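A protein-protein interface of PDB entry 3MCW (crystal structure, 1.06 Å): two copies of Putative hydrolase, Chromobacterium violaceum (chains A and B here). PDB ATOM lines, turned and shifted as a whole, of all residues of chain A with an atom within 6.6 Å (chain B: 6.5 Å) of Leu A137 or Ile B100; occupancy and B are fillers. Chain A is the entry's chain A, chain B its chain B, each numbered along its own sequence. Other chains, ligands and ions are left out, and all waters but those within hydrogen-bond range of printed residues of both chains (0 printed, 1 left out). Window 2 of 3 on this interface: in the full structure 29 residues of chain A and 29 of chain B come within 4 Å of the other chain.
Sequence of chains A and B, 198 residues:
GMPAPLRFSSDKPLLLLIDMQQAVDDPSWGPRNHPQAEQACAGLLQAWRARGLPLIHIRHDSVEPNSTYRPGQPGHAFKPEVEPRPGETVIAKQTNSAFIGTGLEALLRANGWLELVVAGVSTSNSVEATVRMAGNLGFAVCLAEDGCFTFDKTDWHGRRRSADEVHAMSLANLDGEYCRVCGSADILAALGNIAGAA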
ATOM      1  N   PHE A  99     -16.093   9.414  15.561  1.00  0.00           N
ATOM      2  CA  PHE A  99     -15.851  10.029  14.271  1.00  0.00           C
ATOM      3  C   PHE A  99     -14.862  11.203  14.309  1.00  0.00           C
ATOM      4  O   PHE A  99     -14.229  11.532  13.299  1.00  0.00           O
ATOM      5  CB  PHE A  99     -17.160  10.520  13.653  1.00  0.00           C
ATOM      6  CG  PHE A  99     -18.092   9.406  13.290  1.00  0.00           C
ATOM      7  CD1 PHE A  99     -17.983   8.732  12.069  1.00  0.00           C
ATOM      8  CD2 PHE A  99     -19.074   8.985  14.164  1.00  0.00           C
ATOM      9  CE1 PHE A  99     -18.805   7.702  11.724  1.00  0.00           C
ATOM     10  CE2 PHE A  99     -19.899   7.950  13.833  1.00  0.00           C
ATOM     11  CZ  PHE A  99     -19.776   7.298  12.603  1.00  0.00           C
ATOM     12  N   GLU A 105     -15.308   7.914   9.424  1.00  0.00           N
ATOM     13  CA  GLU A 105     -16.327   8.093   8.404  1.00  0.00           C
ATOM     14  C   GLU A 105     -15.794   7.785   6.994  1.00  0.00           C
ATOM     15  O   GLU A 105     -16.430   7.058   6.219  1.00  0.00           O
ATOM     16  CB  GLU A 105     -16.930   9.502   8.423  1.00  0.00           C
ATOM     17  CG  GLU A 105     -18.037   9.664   7.407  1.00  0.00           C
ATOM     18  CD  GLU A 105     -18.628  11.062   7.317  1.00  0.00           C
ATOM     19  OE1 GLU A 105     -18.161  11.975   8.019  1.00  0.00           O
ATOM     20  OE2 GLU A 105     -19.576  11.221   6.527  1.00  0.00           O
ATOM     21  N   ARG A 109     -17.120   4.800   4.434  1.00  0.00           N
ATOM     22  CA  ARG A 109     -17.688   5.111   3.123  1.00  0.00           C
ATOM     23  C   ARG A 109     -16.851   4.514   1.979  1.00  0.00           C
ATOM     24  O   ARG A 109     -17.404   4.038   1.005  1.00  0.00           O
ATOM     25  CB  ARG A 109     -17.849   6.607   2.926  1.00  0.00           C
ATOM     26  CG  ARG A 109     -18.844   7.254   3.908  1.00  0.00           C
ATOM     27  CD  ARG A 109     -19.173   8.658   3.485  1.00  0.00           C
ATOM     28  NE  ARG A 109     -20.033   9.359   4.429  1.00  0.00           N
ATOM     29  CZ  ARG A 109     -21.313   9.133   4.580  1.00  0.00           C
ATOM     30  NH1 ARG A 109     -21.960   8.261   3.822  1.00  0.00           N
ATOM     31  NH2 ARG A 109     -21.948   9.806   5.530  1.00  0.00           N
ATOM     32  N   ARG A 132     -25.352   9.140  17.841  1.00  0.00           N
ATOM     33  CA  ARG A 132     -26.063  10.327  17.350  1.00  0.00           C
ATOM     34  C   ARG A 132     -25.389  10.820  16.075  1.00  0.00           C
ATOM     35  O   ARG A 132     -26.086  11.146  15.102  1.00  0.00           O
ATOM     36  CB  ARG A 132     -26.151  11.431  18.387  1.00  0.00           C
ATOM     37  CG  ARG A 132     -27.128  11.172  19.511  1.00  0.00           C
ATOM     38  CD  ARG A 132     -27.283  12.390  20.410  1.00  0.00           C
ATOM     39  NE  ARG A 132     -28.163  12.207  21.557  1.00  0.00           N
ATOM     40  CZ  ARG A 132     -29.197  12.997  21.857  1.00  0.00           C
ATOM     41  NH1 ARG A 132     -29.610  13.965  21.077  1.00  0.00           N
ATOM     42  NH2 ARG A 132     -29.770  12.851  23.043  1.00  0.00           N
ATOM     43  N   MET A 133     -24.065  10.915  16.080  1.00  0.00           N
ATOM     44  CA  MET A 133     -23.372  11.340  14.848  1.00  0.00           C
ATOM     45  C   MET A 133     -23.543  10.351  13.728  1.00  0.00           C
ATOM     46  O   MET A 133     -23.803  10.749  12.590  1.00  0.00           O
ATOM     47  CB  MET A 133     -21.887  11.614  15.070  1.00  0.00           C
ATOM     48  CG  MET A 133     -21.648  12.888  15.720  1.00  0.00           C
ATOM     49  SD  MET A 133     -19.779  13.464  15.675  1.00  0.00           S
ATOM     50  CE  MET A 133     -19.469  13.501  13.752  1.00  0.00           C
ATOM     51  N   ALA A 134     -23.402   9.057  14.013  1.00  0.00           N
ATOM     52  CA  ALA A 134     -23.570   8.060  12.954  1.00  0.00           C
ATOM     53  C   ALA A 134     -24.916   8.175  12.263  1.00  0.00           C
ATOM     54  O   ALA A 134     -24.999   8.140  11.031  1.00  0.00           O
ATOM     55  CB  ALA A 134     -23.370   6.651  13.508  1.00  0.00           C
ATOM     56  N   GLY A 135     -25.983   8.249  13.043  1.00  0.00           N
ATOM     57  CA  GLY A 135     -27.303   8.325  12.452  1.00  0.00           C
ATOM     58  C   GLY A 135     -27.476   9.598  11.626  1.00  0.00           C
ATOM     59  O   GLY A 135     -27.968   9.574  10.495  1.00  0.00           O
ATOM     60  N   ASN A 136     -27.002  10.727  12.157  1.00  0.00           N
ATOM     61  CA  ASN A 136     -27.140  11.977  11.417  1.00  0.00           C
ATOM     62  C   ASN A 136     -26.270  12.041  10.166  1.00  0.00           C
ATOM     63  O   ASN A 136     -26.621  12.729   9.212  1.00  0.00           O
ATOM     64  CB  ASN A 136     -26.840  13.192  12.316  1.00  0.00           C
ATOM     65  CG  ASN A 136     -27.919  13.550  13.356  1.00  0.00           C
ATOM     66  OD1 ASN A 136     -27.746  14.545  14.050  1.00  0.00           O
ATOM     67  ND2 ASN A 136     -28.995  12.829  13.448  1.00  0.00           N
ATOM     68  N   LEU A 137     -25.157  11.307  10.160  1.00  0.00           N
ATOM     69  CA  LEU A 137     -24.302  11.191   8.973  1.00  0.00           C
ATOM     70  C   LEU A 137     -24.912  10.266   7.913  1.00  0.00           C
ATOM     71  O   LEU A 137     -24.390  10.184   6.805  1.00  0.00           O
ATOM     72  CB  LEU A 137     -22.901  10.702   9.360  1.00  0.00           C
ATOM     73  CG  LEU A 137     -22.023  11.728  10.096  1.00  0.00           C
ATOM     74  CD1 LEU A 137     -20.769  11.047  10.637  1.00  0.00           C
ATOM     75  CD2 LEU A 137     -21.653  12.925   9.210  1.00  0.00           C
ATOM     76  N   GLY A 138     -25.973   9.549   8.232  1.00  0.00           N
ATOM     77  CA  GLY A 138     -26.673   8.683   7.292  1.00  0.00           C
ATOM     78  C   GLY A 138     -26.346   7.210   7.357  1.00  0.00           C
ATOM     79  O   GLY A 138     -26.692   6.465   6.469  1.00  0.00           O
ATOM     80  N   PHE A 139     -25.640   6.784   8.397  1.00  0.00           N
ATOM     81  CA  PHE A 139     -25.402   5.348   8.616  1.00  0.00           C
ATOM     82  C   PHE A 139     -26.645   4.728   9.214  1.00  0.00           C
ATOM     83  O   PHE A 139     -27.401   5.351   9.960  1.00  0.00           O
ATOM     84  CB  PHE A 139     -24.213   5.157   9.554  1.00  0.00           C
ATOM     85  CG  PHE A 139     -22.938   5.590   8.934  1.00  0.00           C
ATOM     86  CD1 PHE A 139     -22.225   4.722   8.145  1.00  0.00           C
ATOM     87  CD2 PHE A 139     -22.423   6.855   9.145  1.00  0.00           C
ATOM     88  CE1 PHE A 139     -21.072   5.117   7.529  1.00  0.00           C
ATOM     89  CE2 PHE A 139     -21.249   7.277   8.523  1.00  0.00           C
ATOM     90  CZ  PHE A 139     -20.583   6.400   7.699  1.00  0.00           C
ATOM     91  N   ALA B  92     -29.911  26.631   7.718  1.00  0.00           N
ATOM     92  CA  ALA B  92     -30.884  25.574   7.751  1.00  0.00           C
ATOM     93  C   ALA B  92     -30.190  24.221   7.838  1.00  0.00           C
ATOM     94  O   ALA B  92     -29.146  24.015   7.225  1.00  0.00           O
ATOM     95  CB  ALA B  92     -31.769  25.648   6.533  1.00  0.00           C
ATOM     96  N   LYS B  93     -30.819  23.288   8.538  1.00  0.00           N
ATOM     97  CA  LYS B  93     -30.313  21.932   8.674  1.00  0.00           C
ATOM     98  C   LYS B  93     -31.422  20.951   8.383  1.00  0.00           C
ATOM     99  O   LYS B  93     -32.610  21.263   8.493  1.00  0.00           O
ATOM    100  CB  LYS B  93     -29.736  21.707  10.094  1.00  0.00           C
ATOM    101  CG  LYS B  93     -30.781  21.669  11.187  1.00  0.00           C
ATOM    102  CD  LYS B  93     -30.128  21.523  12.557  1.00  0.00           C
ATOM    103  CE  LYS B  93     -31.096  21.560  13.708  1.00  0.00           C
ATOM    104  NZ  LYS B  93     -32.022  20.431  13.723  1.00  0.00           N
ATOM    105  N   GLN B  94     -31.022  19.725   8.033  1.00  0.00           N
ATOM    106  CA  GLN B  94     -31.980  18.647   7.749  1.00  0.00           C
ATOM    107  C   GLN B  94     -31.869  17.468   8.711  1.00  0.00           C
ATOM    108  O   GLN B  94     -32.641  16.543   8.585  1.00  0.00           O
ATOM    109  CB  GLN B  94     -31.828  18.160   6.299  1.00  0.00           C
ATOM    110  CG  GLN B  94     -32.116  19.240   5.276  1.00  0.00           C
ATOM    111  CD  GLN B  94     -31.982  18.772   3.854  1.00  0.00           C
ATOM    112  OE1 GLN B  94     -32.934  18.270   3.252  1.00  0.00           O
ATOM    113  NE2 GLN B  94     -30.805  18.977   3.286  1.00  0.00           N
ATOM    114  N   THR B  95     -30.899  17.487   9.608  1.00  0.00           N
ATOM    115  CA  THR B  95     -30.735  16.479  10.644  1.00  0.00           C
ATOM    116  C   THR B  95     -30.668  17.148  11.993  1.00  0.00           C
ATOM    117  O   THR B  95     -30.777  18.357  12.118  1.00  0.00           O
ATOM    118  CB  THR B  95     -29.462  15.622  10.463  1.00  0.00           C
ATOM    119  OG1 THR B  95     -29.650  14.398  11.134  1.00  0.00           O
ATOM    120  CG2 THR B  95     -28.282  16.223  11.167  1.00  0.00           C
ATOM    121  N   SER B  97     -28.140  17.532  14.373  1.00  0.00           N
ATOM    122  CA  SER B  97     -27.012  18.396  14.631  1.00  0.00           C
ATOM    123  C   SER B  97     -26.883  19.543  13.624  1.00  0.00           C
ATOM    124  O   SER B  97     -26.883  19.314  12.424  1.00  0.00           O
ATOM    125  CB  SER B  97     -25.726  17.595  14.625  1.00  0.00           C
ATOM    126  OG  SER B  97     -24.637  18.514  14.689  1.00  0.00           O
ATOM    127  N   ALA B  98     -26.691  20.747  14.141  1.00  0.00           N
ATOM    128  CA  ALA B  98     -26.522  21.934  13.306  1.00  0.00           C
ATOM    129  C   ALA B  98     -25.255  21.934  12.472  1.00  0.00           C
ATOM    130  O   ALA B  98     -25.123  22.777  11.602  1.00  0.00           O
ATOM    131  CB  ALA B  98     -26.568  23.202  14.184  1.00  0.00           C
ATOM    132  N   PHE B  99     -24.336  21.002  12.749  1.00  0.00           N
ATOM    133  CA  PHE B  99     -23.082  20.921  11.995  1.00  0.00           C
ATOM    134  C   PHE B  99     -23.186  20.063  10.734  1.00  0.00           C
ATOM    135  O   PHE B  99     -22.386  20.227   9.814  1.00  0.00           O
ATOM    136  CB  PHE B  99     -21.971  20.369  12.890  1.00  0.00           C
ATOM    137  CG  PHE B  99     -21.587  21.299  13.994  1.00  0.00           C
ATOM    138  CD1 PHE B  99     -20.682  22.304  13.741  1.00  0.00           C
ATOM    139  CD2 PHE B  99     -22.150  21.201  15.243  1.00  0.00           C
ATOM    140  CE1 PHE B  99     -20.339  23.203  14.718  1.00  0.00           C
ATOM    141  CE2 PHE B  99     -21.815  22.084  16.225  1.00  0.00           C
ATOM    142  CZ  PHE B  99     -20.898  23.094  15.958  1.00  0.00           C
ATOM    143  N   ILE B 100     -24.114  19.123  10.693  1.00  0.00           N
ATOM    144  CA  ILE B 100     -24.074  18.113   9.635  1.00  0.00           C
ATOM    145  C   ILE B 100     -24.784  18.632   8.390  1.00  0.00           C
ATOM    146  O   ILE B 100     -25.972  18.957   8.411  1.00  0.00           O
ATOM    147  CB  ILE B 100     -24.611  16.760  10.131  1.00  0.00           C
ATOM    148  CG1 ILE B 100     -23.571  16.207  11.145  1.00  0.00           C
ATOM    149  CG2 ILE B 100     -24.830  15.800   8.969  1.00  0.00           C
ATOM    150  CD1 ILE B 100     -23.905  14.964  11.808  1.00  0.00           C
ATOM    151  N   GLY B 101     -24.027  18.695   7.300  1.00  0.00           N
ATOM    152  CA  GLY B 101     -24.539  19.135   6.011  1.00  0.00           C
ATOM    153  C   GLY B 101     -24.711  20.628   5.859  1.00  0.00           C
ATOM    154  O   GLY B 101     -25.244  21.048   4.852  1.00  0.00           O
ATOM    155  N   THR B 102     -24.240  21.457   6.801  1.00  0.00           N
ATOM    156  CA  THR B 102     -24.595  22.890   6.844  1.00  0.00           C
ATOM    157  C   THR B 102     -23.424  23.866   6.580  1.00  0.00           C
ATOM    158  O   THR B 102     -23.638  25.060   6.377  1.00  0.00           O
ATOM    159  CB  THR B 102     -25.125  23.232   8.239  1.00  0.00           C
ATOM    160  OG1 THR B 102     -24.072  22.972   9.163  1.00  0.00           O
ATOM    161  CG2 THR B 102     -26.369  22.410   8.640  1.00  0.00           C
ATOM    162  N   GLY B 103     -22.196  23.357   6.682  1.00  0.00           N
ATOM    163  CA  GLY B 103     -21.012  24.213   6.644  1.00  0.00           C
ATOM    164  C   GLY B 103     -20.774  25.092   7.884  1.00  0.00           C
ATOM    165  O   GLY B 103     -19.907  25.949   7.851  1.00  0.00           O
ATOM    166  N   LEU B 104     -21.511  24.880   8.973  1.00  0.00           N
ATOM    167  CA  LEU B 104     -21.425  25.690  10.195  1.00  0.00           C
ATOM    168  C   LEU B 104     -20.010  25.716  10.741  1.00  0.00           C
ATOM    169  O   LEU B 104     -19.491  26.781  11.084  1.00  0.00           O
ATOM    170  CB  LEU B 104     -22.407  25.180  11.238  1.00  0.00           C
ATOM    171  CG  LEU B 104     -22.388  25.881  12.587  1.00  0.00           C
ATOM    172  CD1 LEU B 104     -22.731  27.350  12.449  1.00  0.00           C
ATOM    173  CD2 LEU B 104     -23.317  25.167  13.562  1.00  0.00           C
ATOM    174  N   MET B 133     -21.615  17.580  19.546  1.00  0.00           N
ATOM    175  CA  MET B 133     -20.651  17.749  18.467  1.00  0.00           C
ATOM    176  C   MET B 133     -19.806  18.997  18.647  1.00  0.00           C
ATOM    177  O   MET B 133     -18.602  18.965  18.428  1.00  0.00           O
ATOM    178  CB  MET B 133     -21.289  17.767  17.113  1.00  0.00           C
ATOM    179  CG  MET B 133     -21.657  16.414  16.630  1.00  0.00           C
ATOM    180  SD  MET B 133     -22.205  16.369  14.755  1.00  0.00           S
ATOM    181  CE  MET B 133     -20.549  17.025  13.928  1.00  0.00           C
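OG1 of Thr B95 lies within hydrogen-bond range of ND2 of Asn A136 (2.9 Å). The side-chain amide oxygen (OD1) of Asn A136 sits at hydrogen-bond distance from the backbone NH (N) of Ser B97 (3.0 Å).
OG of Ser B97 sits close to N of Phe B99 (3.2 Å). The guanidinium group of Arg A109 sits at hydrogen-bond distance from the backbone carbonyl oxygen of Leu A137. NZ of Lys B93 sits at hydrogen-bond distance from O of Thr B95, at 2.9 Å. The side-chain hydroxyl of Ser B97 lies within hydrogen-bond range of the side-chain sulfur of Met B133 (3.2 Å).
Met A133 touches Met B133 (SD to CG, 3.6 Å). Asn A136 touches Ile B100 (CB to CD1, 3.5 Å). CD1 of Ile B100 touches CD2 of Leu A137 (3.997 Å).
Arg A132 touches none of the printed residues of chain B. Of the printed residues of chain B, Met A133 touches Met B133 (3.6 Å). Ala A134 touches none of the printed residues of chain B. Of the printed residues of chain B, Leu A137 touches Ile B100 (3.997 Å). Of the printed residues of chain A, Thr B95 touches Asn A136. Of the printed residues of chain A, Ser B97 touches Asn A136 (3.0 Å). Of the printed residues of chain A, Ile B100 touches Asn A136 (3.5 Å) and Leu A137 (3.997 Å). Of the printed residues of chain A, Met B133 touches Met A133 (3.6 Å). The nearest printed residue of chain B that does not touch Leu A137 is Thr B95 (5.5 Å). The nearest printed residue of chain B that does not touch Met A133 is Ile B100 (4.3 Å).
Printed residues of chain A that touch a printed residue of chain B: Met A133, Asn A136 and Leu A137. Of the 13 printed residues of chain B, 4 touch a printed residue of chain A. Hydrophobic or aromatic side chains of chain B that line the printed part of chain A: Ile B100 and Met B133.
Met A133 touches its own counterpart, Met B133. 2 positions are printed for both chains. Of the 5 pairs that touch across the chains among the printed residues, 1 has its exchanged pair printed and touching as well.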
